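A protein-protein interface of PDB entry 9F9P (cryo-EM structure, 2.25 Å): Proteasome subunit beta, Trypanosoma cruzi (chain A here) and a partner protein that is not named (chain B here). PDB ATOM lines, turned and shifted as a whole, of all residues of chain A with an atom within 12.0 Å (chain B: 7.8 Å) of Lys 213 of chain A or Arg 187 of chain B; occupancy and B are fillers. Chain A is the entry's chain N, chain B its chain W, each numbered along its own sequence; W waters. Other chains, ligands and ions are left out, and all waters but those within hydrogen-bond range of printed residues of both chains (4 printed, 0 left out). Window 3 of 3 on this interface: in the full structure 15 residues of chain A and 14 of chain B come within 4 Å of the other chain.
Lys 213 of chain A touches just one residue of chain B: Arg 187 (3.6 Å). Arg 187 of chain B touches one residue of chain A. No residue of chain A comes within 4 Å of Gly 173 of chain B. Of the printed residues of chain A, Phe 175 of chain B touches Arg 218. No residue of chain A comes within 4 Å of Leu 176 of chain B. No residue of chain A comes within 4 Å of Thr 178 of chain B. No residue of chain A comes within 4 Å of Thr 185 of chain B. No residue of chain A comes within 4 Å of Asp 186 of chain B. No residue of chain A comes within 4 Å of Leu 188 of chain B. Of the printed residues of chain B, Gly 208 of chain A touches Pro 189 (3.97 Å). Of the printed residues of chain A, His 143 of chain B touches Arg 218 (3.3 Å). Of the printed residues of chain B, Arg 218 of chain A touches His 143 and Phe 175. Of the printed residues of chain A, Pro 189 of chain B touches Gly 208 (3.97 Å). The nearest residue of chain B that does not touch Lys 213 of chain A is Pro 174 of chain B (5.3 Å). The nearest residue of chain A that does not touch Arg 187 of chain B is Thr 214 of chain A (4.4 Å). The nearest printed residue of chain A that does not touch Pro 189 of chain B is Phe 209 of chain A (4.2 Å).
Water W1 lies within hydrogen-bond range of the side-chain carboxylate (OE1) of Glu 172 of chain B (2.7 Å) and the guanidinium group (NH1) of Arg 218 of chain A (2.8 Å). Water W2 lies within hydrogen-bond range of O of Gly 208 of chain A and O of Arg 187 of chain B. Water W3 lies within hydrogen-bond range of the guanidinium group of Arg 174 of chain A and the backbone carbonyl oxygen of Phe 190 of chain B. Water W4 bridges O of Pro 174 of chain B (3.2 Å) and NZ of Lys 213 of chain A (3.4 Å).
The backbone NH (N) of Lys 213 of chain A sits at hydrogen-bond distance from the side-chain sulfur (SG) of Cys 210 of chain A. O of Pro 189 of chain B lies within hydrogen-bond range of N of Val 73 of chain B, at 3.1 Å. The backbone NH (N) of Phe 175 of chain B lies within hydrogen-bond range of the backbone carbonyl oxygen (O) of Gly 168 of chain B (3.0 Å). The backbone carbonyl oxygen (O) of Pro 174 of chain B lies within hydrogen-bond range of the guanidinium group (NH2) of Arg 187 of chain B, 3.4 Å away.
O of Gly 208 of chain A touches CD of Pro 189 of chain B (3.97 Å). Lys 213 of chain A touches Arg 187 of chain B (O to CD, 3.6 Å). NH1 of Arg 218 of chain A touches CG of His 143 of chain B, at 3.3 Å. NH1 of Arg 218 of chain A touches CE2 of Phe 175 of chain B, at 3.7 Å.
Of the 16 printed residues of chain A, 3 touch a printed residue of chain B. Hydrophobic or aromatic side chains of chain B that line the printed part of chain A: His 143, Phe 175 and Pro 189. Among the printed residues, 4 pairs touch across the chains. Among the printed residues, no Asp or Glu carboxylate lies within 4 Å of a Lys or Arg side-chain nitrogen of the other chain.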
ATOM      1  N   ARG A 174      -0.023  16.829  12.682  1.00  0.00           N
ATOM      2  CA  ARG A 174       0.521  16.285  13.922  1.00  0.00           C
ATOM      3  C   ARG A 174       1.738  15.378  13.797  1.00  0.00           C
ATOM      4  O   ARG A 174       2.371  15.141  14.815  1.00  0.00           O
ATOM      5  CB  ARG A 174      -0.579  15.547  14.688  1.00  0.00           C
ATOM      6  CG  ARG A 174      -1.821  16.393  15.015  1.00  0.00           C
ATOM      7  CD  ARG A 174      -1.514  17.309  16.183  1.00  0.00           C
ATOM      8  NE  ARG A 174      -2.454  18.386  16.425  1.00  0.00           N
ATOM      9  CZ  ARG A 174      -2.417  19.162  17.516  1.00  0.00           C
ATOM     10  NH1 ARG A 174      -1.563  18.897  18.493  1.00  0.00           N
ATOM     11  NH2 ARG A 174      -3.282  20.149  17.665  1.00  0.00           N
ATOM     12  N   TRP A 204      -5.843  27.229   9.809  1.00  0.00           N
ATOM     13  CA  TRP A 204      -4.845  27.870  10.646  1.00  0.00           C
ATOM     14  C   TRP A 204      -5.355  29.142  11.311  1.00  0.00           C
ATOM     15  O   TRP A 204      -4.555  29.819  11.942  1.00  0.00           O
ATOM     16  CB  TRP A 204      -3.599  28.169   9.809  1.00  0.00           C
ATOM     17  CG  TRP A 204      -2.954  26.914   9.321  1.00  0.00           C
ATOM     18  CD1 TRP A 204      -3.188  26.244   8.144  1.00  0.00           C
ATOM     19  CD2 TRP A 204      -2.036  26.118  10.086  1.00  0.00           C
ATOM     20  NE1 TRP A 204      -2.469  25.076   8.138  1.00  0.00           N
ATOM     21  CE2 TRP A 204      -1.743  24.985   9.304  1.00  0.00           C
ATOM     22  CE3 TRP A 204      -1.487  26.243  11.364  1.00  0.00           C
ATOM     23  CZ2 TRP A 204      -0.857  24.011   9.742  1.00  0.00           C
ATOM     24  CZ3 TRP A 204      -0.584  25.289  11.804  1.00  0.00           C
ATOM     25  CH2 TRP A 204      -0.288  24.179  11.000  1.00  0.00           C
ATOM     26  N   GLU A 205      -6.638  29.488  11.177  1.00  0.00           N
ATOM     27  CA  GLU A 205      -7.089  30.832  11.498  1.00  0.00           C
ATOM     28  C   GLU A 205      -8.114  30.862  12.618  1.00  0.00           C
ATOM     29  O   GLU A 205      -8.881  31.814  12.703  1.00  0.00           O
ATOM     30  CB  GLU A 205      -7.695  31.475  10.243  1.00  0.00           C
ATOM     31  CG  GLU A 205      -6.642  32.044   9.296  1.00  0.00           C
ATOM     32  CD  GLU A 205      -6.741  31.547   7.862  1.00  0.00           C
ATOM     33  OE1 GLU A 205      -6.458  30.334   7.631  1.00  0.00           O
ATOM     34  OE2 GLU A 205      -7.110  32.361   6.973  1.00  0.00           O
ATOM     35  N   TYR A 206      -8.111  29.887  13.520  1.00  0.00           N
ATOM     36  CA  TYR A 206      -9.013  29.937  14.653  1.00  0.00           C
ATOM     37  C   TYR A 206      -8.676  31.149  15.533  1.00  0.00           C
ATOM     38  O   TYR A 206      -7.507  31.480  15.706  1.00  0.00           O
ATOM     39  CB  TYR A 206      -8.904  28.641  15.461  1.00  0.00           C
ATOM     40  CG  TYR A 206      -9.257  27.360  14.731  1.00  0.00           C
ATOM     41  CD1 TYR A 206     -10.459  27.226  14.031  1.00  0.00           C
ATOM     42  CD2 TYR A 206      -8.380  26.276  14.727  1.00  0.00           C
ATOM     43  CE1 TYR A 206     -10.771  26.047  13.379  1.00  0.00           C
ATOM     44  CE2 TYR A 206      -8.688  25.090  14.077  1.00  0.00           C
ATOM     45  CZ  TYR A 206      -9.889  24.972  13.407  1.00  0.00           C
ATOM     46  OH  TYR A 206     -10.191  23.803  12.750  1.00  0.00           O
ATOM     47  N   ASP A 207      -9.683  31.740  16.194  1.00  0.00           N
ATOM     48  CA  ASP A 207      -9.467  32.852  17.124  1.00  0.00           C
ATOM     49  C   ASP A 207      -8.492  32.475  18.245  1.00  0.00           C
ATOM     50  O   ASP A 207      -7.656  33.300  18.623  1.00  0.00           O
ATOM     51  CB  ASP A 207     -10.763  33.371  17.757  1.00  0.00           C
ATOM     52  CG  ASP A 207     -10.526  34.366  18.895  1.00  0.00           C
ATOM     53  OD1 ASP A 207     -10.127  35.525  18.596  1.00  0.00           O
ATOM     54  OD2 ASP A 207     -10.694  33.973  20.089  1.00  0.00           O
ATOM     55  N   GLY A 208      -8.572  31.232  18.738  1.00  0.00           N
ATOM     56  CA  GLY A 208      -7.690  30.732  19.786  1.00  0.00           C
ATOM     57  C   GLY A 208      -6.218  30.544  19.381  1.00  0.00           C
ATOM     58  O   GLY A 208      -5.399  30.245  20.240  1.00  0.00           O
ATOM     59  N   PHE A 209      -5.858  30.777  18.117  1.00  0.00           N
ATOM     60  CA  PHE A 209      -4.477  30.686  17.687  1.00  0.00           C
ATOM     61  C   PHE A 209      -3.831  32.059  17.577  1.00  0.00           C
ATOM     62  O   PHE A 209      -2.676  32.164  17.142  1.00  0.00           O
ATOM     63  CB  PHE A 209      -4.382  29.992  16.313  1.00  0.00           C
ATOM     64  CG  PHE A 209      -4.524  28.493  16.315  1.00  0.00           C
ATOM     65  CD1 PHE A 209      -4.785  27.792  17.482  1.00  0.00           C
ATOM     66  CD2 PHE A 209      -4.409  27.782  15.127  1.00  0.00           C
ATOM     67  CE1 PHE A 209      -4.935  26.416  17.466  1.00  0.00           C
ATOM     68  CE2 PHE A 209      -4.547  26.403  15.113  1.00  0.00           C
ATOM     69  CZ  PHE A 209      -4.847  25.724  16.272  1.00  0.00           C
ATOM     70  N   CYS A 210      -4.550  33.107  17.963  1.00  0.00           N
ATOM     71  CA  CYS A 210      -4.071  34.468  17.771  1.00  0.00           C
ATOM     72  C   CYS A 210      -2.965  34.861  18.764  1.00  0.00           C
ATOM     73  O   CYS A 210      -2.819  34.261  19.832  1.00  0.00           O
ATOM     74  CB  CYS A 210      -5.237  35.443  17.875  1.00  0.00           C
ATOM     75  SG  CYS A 210      -5.530  36.022  19.568  1.00  0.00           S
ATOM     76  N   PHE A 211      -2.209  35.909  18.393  1.00  0.00           N
ATOM     77  CA  PHE A 211      -0.973  36.318  19.066  1.00  0.00           C
ATOM     78  C   PHE A 211      -1.221  36.707  20.524  1.00  0.00           C
ATOM     79  O   PHE A 211      -0.500  36.272  21.412  1.00  0.00           O
ATOM     80  CB  PHE A 211      -0.313  37.457  18.277  1.00  0.00           C
ATOM     81  CG  PHE A 211       1.081  37.822  18.675  1.00  0.00           C
ATOM     82  CD1 PHE A 211       1.326  38.529  19.846  1.00  0.00           C
ATOM     83  CD2 PHE A 211       2.159  37.496  17.853  1.00  0.00           C
ATOM     84  CE1 PHE A 211       2.630  38.861  20.216  1.00  0.00           C
ATOM     85  CE2 PHE A 211       3.463  37.844  18.220  1.00  0.00           C
ATOM     86  CZ  PHE A 211       3.697  38.519  19.407  1.00  0.00           C
ATOM     87  N   GLU A 212      -2.314  37.428  20.788  1.00  0.00           N
ATOM     88  CA  GLU A 212      -2.637  37.858  22.144  1.00  0.00           C
ATOM     89  C   GLU A 212      -2.972  36.664  23.063  1.00  0.00           C
ATOM     90  O   GLU A 212      -2.439  36.579  24.165  1.00  0.00           O
ATOM     91  CB  GLU A 212      -3.738  38.913  22.082  1.00  0.00           C
ATOM     92  CG  GLU A 212      -4.191  39.387  23.459  1.00  0.00           C
ATOM     93  CD  GLU A 212      -5.700  39.358  23.701  1.00  0.00           C
ATOM     94  OE1 GLU A 212      -6.429  40.135  23.028  1.00  0.00           O
ATOM     95  OE2 GLU A 212      -6.153  38.542  24.552  1.00  0.00           O
ATOM     96  N   LYS A 213      -3.816  35.723  22.628  1.00  0.00           N
ATOM     97  CA  LYS A 213      -4.250  34.628  23.491  1.00  0.00           C
ATOM     98  C   LYS A 213      -3.154  33.607  23.802  1.00  0.00           C
ATOM     99  O   LYS A 213      -3.163  33.031  24.876  1.00  0.00           O
ATOM    100  CB  LYS A 213      -5.353  33.796  22.836  1.00  0.00           C
ATOM    101  CG  LYS A 213      -6.696  34.467  22.686  1.00  0.00           C
ATOM    102  CD  LYS A 213      -7.751  33.906  23.599  1.00  0.00           C
ATOM    103  CE  LYS A 213      -9.132  34.294  23.123  1.00  0.00           C
ATOM    104  NZ  LYS A 213     -10.056  34.416  24.267  1.00  0.00           N
ATOM    105  N   THR A 214      -2.234  33.373  22.871  1.00  0.00           N
ATOM    106  CA  THR A 214      -1.163  32.397  23.037  1.00  0.00           C
ATOM    107  C   THR A 214       0.060  32.974  23.772  1.00  0.00           C
ATOM    108  O   THR A 214       0.987  32.228  24.108  1.00  0.00           O
ATOM    109  CB  THR A 214      -0.771  31.817  21.663  1.00  0.00           C
ATOM    110  OG1 THR A 214      -0.386  32.868  20.764  1.00  0.00           O
ATOM    111  CG2 THR A 214      -1.903  31.038  21.013  1.00  0.00           C
ATOM    112  N   ALA A 215       0.082  34.288  24.037  1.00  0.00           N
ATOM    113  CA  ALA A 215       1.188  34.928  24.748  1.00  0.00           C
ATOM    114  C   ALA A 215       1.387  34.375  26.160  1.00  0.00           C
ATOM    115  O   ALA A 215       0.439  34.146  26.887  1.00  0.00           O
ATOM    116  CB  ALA A 215       0.984  36.425  24.792  1.00  0.00           C
ATOM    117  N   ILE A 216       2.652  34.191  26.554  1.00  0.00           N
ATOM    118  CA  ILE A 216       2.999  33.646  27.866  1.00  0.00           C
ATOM    119  C   ILE A 216       2.934  34.718  28.956  1.00  0.00           C
ATOM    120  O   ILE A 216       2.579  34.393  30.071  1.00  0.00           O
ATOM    121  CB  ILE A 216       4.404  32.997  27.826  1.00  0.00           C
ATOM    122  CG1 ILE A 216       4.534  31.907  26.747  1.00  0.00           C
ATOM    123  CG2 ILE A 216       4.781  32.463  29.191  1.00  0.00           C
ATOM    124  CD1 ILE A 216       3.621  30.723  26.948  1.00  0.00           C
ATOM    125  N   ILE A 217       3.344  35.955  28.642  1.00  0.00           N
ATOM    126  CA  ILE A 217       3.322  37.095  29.550  1.00  0.00           C
ATOM    127  C   ILE A 217       2.428  38.212  28.971  1.00  0.00           C
ATOM    128  O   ILE A 217       2.621  38.662  27.834  1.00  0.00           O
ATOM    129  CB  ILE A 217       4.761  37.594  29.797  1.00  0.00           C
ATOM    130  CG1 ILE A 217       5.650  36.567  30.500  1.00  0.00           C
ATOM    131  CG2 ILE A 217       4.780  38.914  30.552  1.00  0.00           C
ATOM    132  CD1 ILE A 217       7.146  36.902  30.396  1.00  0.00           C
ATOM    133  N   ARG A 218       1.499  38.707  29.811  1.00  0.00           N
ATOM    134  CA  ARG A 218       0.350  39.500  29.386  1.00  0.00           C
ATOM    135  C   ARG A 218       0.618  40.994  29.620  1.00  0.00           C
ATOM    136  O   ARG A 218      -0.357  41.766  29.481  1.00  0.00           O
ATOM    137  CB  ARG A 218      -0.922  39.117  30.158  1.00  0.00           C
ATOM    138  CG  ARG A 218      -1.115  37.624  30.420  1.00  0.00           C
ATOM    139  CD  ARG A 218      -2.082  36.924  29.472  1.00  0.00           C
ATOM    140  NE  ARG A 218      -2.886  35.892  30.132  1.00  0.00           N
ATOM    141  CZ  ARG A 218      -3.808  36.119  31.071  1.00  0.00           C
ATOM    142  NH1 ARG A 218      -4.507  35.115  31.566  1.00  0.00           N
ATOM    143  NH2 ARG A 218      -4.043  37.346  31.507  1.00  0.00           N
ATOM    144  OXT ARG A 218       1.788  41.337  29.933  1.00  0.00           O
ATOM    145  N   VAL B  73     -13.176  24.540  24.346  1.00  0.00           N
ATOM    146  CA  VAL B  73     -13.874  25.793  24.544  1.00  0.00           C
ATOM    147  C   VAL B  73     -15.049  25.914  23.562  1.00  0.00           C
ATOM    148  O   VAL B  73     -14.881  25.763  22.363  1.00  0.00           O
ATOM    149  CB  VAL B  73     -12.904  26.979  24.375  1.00  0.00           C
ATOM    150  CG1 VAL B  73     -13.592  28.311  24.342  1.00  0.00           C
ATOM    151  CG2 VAL B  73     -11.904  27.038  25.498  1.00  0.00           C
ATOM    152  N   HIS B 143      -6.249  31.923  35.467  1.00  0.00           N
ATOM    153  CA  HIS B 143      -4.824  32.190  35.326  1.00  0.00           C
ATOM    154  C   HIS B 143      -4.052  32.067  36.648  1.00  0.00           C
ATOM    155  O   HIS B 143      -2.863  31.762  36.627  1.00  0.00           O
ATOM    156  CB  HIS B 143      -4.553  33.504  34.566  1.00  0.00           C
ATOM    157  CG  HIS B 143      -3.117  33.690  34.142  1.00  0.00           C
ATOM    158  ND1 HIS B 143      -2.200  34.493  34.809  1.00  0.00           N
ATOM    159  CD2 HIS B 143      -2.406  33.118  33.108  1.00  0.00           C
ATOM    160  CE1 HIS B 143      -0.995  34.422  34.215  1.00  0.00           C
ATOM    161  NE2 HIS B 143      -1.102  33.596  33.174  1.00  0.00           N
ATOM    162  N   LEU B 146      -3.459  28.337  37.287  1.00  0.00           N
ATOM    163  CA  LEU B 146      -2.446  27.952  36.328  1.00  0.00           C
ATOM    164  C   LEU B 146      -1.049  28.353  36.762  1.00  0.00           C
ATOM    165  O   LEU B 146      -0.156  27.547  36.681  1.00  0.00           O
ATOM    166  CB  LEU B 146      -2.753  28.549  34.955  1.00  0.00           C
ATOM    167  CG  LEU B 146      -1.730  28.108  33.910  1.00  0.00           C
ATOM    168  CD1 LEU B 146      -1.888  26.609  33.615  1.00  0.00           C
ATOM    169  CD2 LEU B 146      -1.789  28.937  32.634  1.00  0.00           C
ATOM    170  N   GLY B 168     -11.792  26.589  33.184  1.00  0.00           N
ATOM    171  CA  GLY B 168     -12.785  27.276  33.985  1.00  0.00           C
ATOM    172  C   GLY B 168     -13.280  28.557  33.343  1.00  0.00           C
ATOM    173  O   GLY B 168     -12.867  28.856  32.249  1.00  0.00           O
ATOM    174  N   ASP B 170     -14.179  32.771  34.249  1.00  0.00           N
ATOM    175  CA  ASP B 170     -14.137  33.889  35.183  1.00  0.00           C
ATOM    176  C   ASP B 170     -14.531  35.170  34.442  1.00  0.00           C
ATOM    177  O   ASP B 170     -15.102  35.112  33.363  1.00  0.00           O
ATOM    178  CB  ASP B 170     -12.771  33.981  35.868  1.00  0.00           C
ATOM    179  CG  ASP B 170     -11.599  34.213  34.918  1.00  0.00           C
ATOM    180  OD1 ASP B 170     -11.843  34.802  33.819  1.00  0.00           O
ATOM    181  OD2 ASP B 170     -10.452  33.751  35.221  1.00  0.00           O
ATOM    182  N   GLU B 172     -13.091  37.289  32.711  1.00  0.00           N
ATOM    183  CA  GLU B 172     -12.569  37.475  31.357  1.00  0.00           C
ATOM    184  C   GLU B 172     -12.956  36.337  30.399  1.00  0.00           C
ATOM    185  O   GLU B 172     -12.309  36.147  29.379  1.00  0.00           O
ATOM    186  CB  GLU B 172     -11.047  37.577  31.360  1.00  0.00           C
ATOM    187  CG  GLU B 172     -10.472  38.558  32.374  1.00  0.00           C
ATOM    188  CD  GLU B 172      -8.942  38.608  32.421  1.00  0.00           C
ATOM    189  OE1 GLU B 172      -8.312  37.550  32.671  1.00  0.00           O
ATOM    190  OE2 GLU B 172      -8.369  39.708  32.208  1.00  0.00           O
ATOM    191  N   GLY B 173     -13.981  35.540  30.727  1.00  0.00           N
ATOM    192  CA  GLY B 173     -14.466  34.520  29.813  1.00  0.00           C
ATOM    193  C   GLY B 173     -13.818  33.153  30.039  1.00  0.00           C
ATOM    194  O   GLY B 173     -13.148  32.939  31.053  1.00  0.00           O
ATOM    195  N   PRO B 174     -14.074  32.187  29.124  1.00  0.00           N
ATOM    196  CA  PRO B 174     -13.568  30.811  29.229  1.00  0.00           C
ATOM    197  C   PRO B 174     -12.059  30.687  29.094  1.00  0.00           C
ATOM    198  O   PRO B 174     -11.465  31.389  28.319  1.00  0.00           O
ATOM    199  CB  PRO B 174     -14.206  30.108  28.019  1.00  0.00           C
ATOM    200  CG  PRO B 174     -15.422  30.944  27.704  1.00  0.00           C
ATOM    201  CD  PRO B 174     -14.956  32.363  27.959  1.00  0.00           C
ATOM    202  N   PHE B 175     -11.462  29.764  29.805  1.00  0.00           N
ATOM    203  CA  PHE B 175     -10.045  29.573  29.783  1.00  0.00           C
ATOM    204  C   PHE B 175      -9.725  28.087  29.826  1.00  0.00           C
ATOM    205  O   PHE B 175     -10.198  27.404  30.697  1.00  0.00           O
ATOM    206  CB  PHE B 175      -9.478  30.287  31.001  1.00  0.00           C
ATOM    207  CG  PHE B 175      -7.982  30.444  31.072  1.00  0.00           C
ATOM    208  CD1 PHE B 175      -7.167  29.368  31.358  1.00  0.00           C
ATOM    209  CD2 PHE B 175      -7.400  31.677  30.891  1.00  0.00           C
ATOM    210  CE1 PHE B 175      -5.788  29.504  31.401  1.00  0.00           C
ATOM    211  CE2 PHE B 175      -6.022  31.816  30.904  1.00  0.00           C
ATOM    212  CZ  PHE B 175      -5.208  30.725  31.141  1.00  0.00           C
ATOM    213  N   LEU B 176      -8.911  27.595  28.913  1.00  0.00           N
ATOM    214  CA  LEU B 176      -8.486  26.205  28.898  1.00  0.00           C
ATOM    215  C   LEU B 176      -6.976  26.092  28.691  1.00  0.00           C
ATOM    216  O   LEU B 176      -6.433  26.694  27.790  1.00  0.00           O
ATOM    217  CB  LEU B 176      -9.267  25.540  27.770  1.00  0.00           C
ATOM    218  CG  LEU B 176      -8.864  24.104  27.440  1.00  0.00           C
ATOM    219  CD1 LEU B 176      -9.304  23.164  28.557  1.00  0.00           C
ATOM    220  CD2 LEU B 176      -9.504  23.672  26.139  1.00  0.00           C
ATOM    221  N   ALA B 177      -6.294  25.299  29.511  1.00  0.00           N
ATOM    222  CA  ALA B 177      -4.885  25.097  29.289  1.00  0.00           C
ATOM    223  C   ALA B 177      -4.365  23.749  29.752  1.00  0.00           C
ATOM    224  O   ALA B 177      -5.005  23.087  30.524  1.00  0.00           O
ATOM    225  CB  ALA B 177      -4.137  26.163  30.015  1.00  0.00           C
ATOM    226  N   THR B 178      -3.156  23.397  29.313  1.00  0.00           N
ATOM    227  CA  THR B 178      -2.457  22.224  29.802  1.00  0.00           C
ATOM    228  C   THR B 178      -1.245  22.594  30.631  1.00  0.00           C
ATOM    229  O   THR B 178      -0.653  23.624  30.425  1.00  0.00           O
ATOM    230  CB  THR B 178      -1.901  21.353  28.675  1.00  0.00           C
ATOM    231  OG1 THR B 178      -1.090  22.107  27.762  1.00  0.00           O
ATOM    232  CG2 THR B 178      -2.997  20.719  27.852  1.00  0.00           C
ATOM    233  N   THR B 185       3.449  25.458  30.177  1.00  0.00           N
ATOM    234  CA  THR B 185       2.028  25.602  29.891  1.00  0.00           C
ATOM    235  C   THR B 185       1.711  26.024  28.464  1.00  0.00           C
ATOM    236  O   THR B 185       2.572  26.531  27.757  1.00  0.00           O
ATOM    237  CB  THR B 185       1.420  26.684  30.788  1.00  0.00           C
ATOM    238  OG1 THR B 185       2.043  27.941  30.510  1.00  0.00           O
ATOM    239  CG2 THR B 185       1.593  26.309  32.245  1.00  0.00           C
ATOM    240  N   ASP B 186       0.440  25.845  28.096  1.00  0.00           N
ATOM    241  CA  ASP B 186      -0.088  26.146  26.776  1.00  0.00           C
ATOM    242  C   ASP B 186      -1.561  26.461  26.939  1.00  0.00           C
ATOM    243  O   ASP B 186      -2.286  25.667  27.513  1.00  0.00           O
ATOM    244  CB  ASP B 186      -0.004  24.950  25.824  1.00  0.00           C
ATOM    245  CG  ASP B 186       1.406  24.468  25.450  1.00  0.00           C
ATOM    246  OD1 ASP B 186       2.175  25.261  24.792  1.00  0.00           O
ATOM    247  OD2 ASP B 186       1.733  23.290  25.765  1.00  0.00           O
ATOM    248  N   ARG B 187      -1.979  27.642  26.496  1.00  0.00           N
ATOM    249  CA  ARG B 187      -3.374  28.008  26.461  1.00  0.00           C
ATOM    250  C   ARG B 187      -3.915  27.791  25.046  1.00  0.00           C
ATOM    251  O   ARG B 187      -3.339  28.298  24.100  1.00  0.00           O
ATOM    252  CB  ARG B 187      -3.511  29.442  26.954  1.00  0.00           C
ATOM    253  CG  ARG B 187      -4.967  29.859  26.944  1.00  0.00           C
ATOM    254  CD  ARG B 187      -5.265  31.298  27.198  1.00  0.00           C
ATOM    255  NE  ARG B 187      -6.679  31.496  27.049  1.00  0.00           N
ATOM    256  CZ  ARG B 187      -7.273  32.635  27.356  1.00  0.00           C
ATOM    257  NH1 ARG B 187      -6.529  33.648  27.732  1.00  0.00           N
ATOM    258  NH2 ARG B 187      -8.588  32.753  27.273  1.00  0.00           N
ATOM    259  N   LEU B 188      -4.955  26.957  24.864  1.00  0.00           N
ATOM    260  CA  LEU B 188      -5.429  26.587  23.515  1.00  0.00           C
ATOM    261  C   LEU B 188      -6.923  26.394  23.518  1.00  0.00           C
ATOM    262  O   LEU B 188      -7.484  26.177  24.556  1.00  0.00           O
ATOM    263  CB  LEU B 188      -4.768  25.282  23.035  1.00  0.00           C
ATOM    264  CG  LEU B 188      -3.250  25.344  22.755  1.00  0.00           C
ATOM    265  CD1 LEU B 188      -2.572  23.969  22.750  1.00  0.00           C
ATOM    266  CD2 LEU B 188      -2.975  26.036  21.433  1.00  0.00           C
ATOM    267  N   PRO B 189      -7.604  26.377  22.371  1.00  0.00           N
ATOM    268  CA  PRO B 189      -9.022  26.023  22.323  1.00  0.00           C
ATOM    269  C   PRO B 189      -9.492  24.563  22.286  1.00  0.00           C
ATOM    270  O   PRO B 189     -10.681  24.321  22.458  1.00  0.00           O
ATOM    271  CB  PRO B 189      -9.441  26.679  21.030  1.00  0.00           C
ATOM    272  CG  PRO B 189      -8.239  26.631  20.146  1.00  0.00           C
ATOM    273  CD  PRO B 189      -7.049  26.731  21.064  1.00  0.00           C
ATOM    274  N   PHE B 190      -8.568  23.603  22.154  1.00  0.00           N
ATOM    275  CA  PHE B 190      -8.868  22.183  22.337  1.00  0.00           C
ATOM    276  C   PHE B 190      -7.568  21.472  22.670  1.00  0.00           C
ATOM    277  O   PHE B 190      -6.559  21.835  22.119  1.00  0.00           O
ATOM    278  CB  PHE B 190      -9.556  21.618  21.093  1.00  0.00           C
ATOM    279  CG  PHE B 190      -8.808  21.719  19.783  1.00  0.00           C
ATOM    280  CD1 PHE B 190      -8.988  22.809  18.946  1.00  0.00           C
ATOM    281  CD2 PHE B 190      -7.947  20.715  19.357  1.00  0.00           C
ATOM    282  CE1 PHE B 190      -8.291  22.935  17.737  1.00  0.00           C
ATOM    283  CE2 PHE B 190      -7.267  20.816  18.143  1.00  0.00           C
ATOM    284  CZ  PHE B 190      -7.430  21.930  17.338  1.00  0.00           C
ATOM    285  N   VAL B 191      -7.579  20.543  23.622  1.00  0.00           N
ATOM    286  CA  VAL B 191      -6.376  19.844  24.035  1.00  0.00           C
ATOM    287  C   VAL B 191      -6.711  18.405  24.334  1.00  0.00           C
ATOM    288  O   VAL B 191      -7.853  18.103  24.578  1.00  0.00           O
ATOM    289  CB  VAL B 191      -5.731  20.464  25.295  1.00  0.00           C
ATOM    290  CG1 VAL B 191      -5.430  21.917  25.106  1.00  0.00           C
ATOM    291  CG2 VAL B 191      -6.616  20.382  26.519  1.00  0.00           C
HETATM  292  O   HOH W   1      -7.321  35.283  31.570  1.00  0.00           O
HETATM  293  O   HOH W   2      -5.652  30.222  23.019  1.00  0.00           O
HETATM  294  O   HOH W   3      -3.735  21.104  20.716  1.00  0.00           O
HETATM  295  O   HOH W   4     -11.367  31.427  25.090  1.00  0.00           O
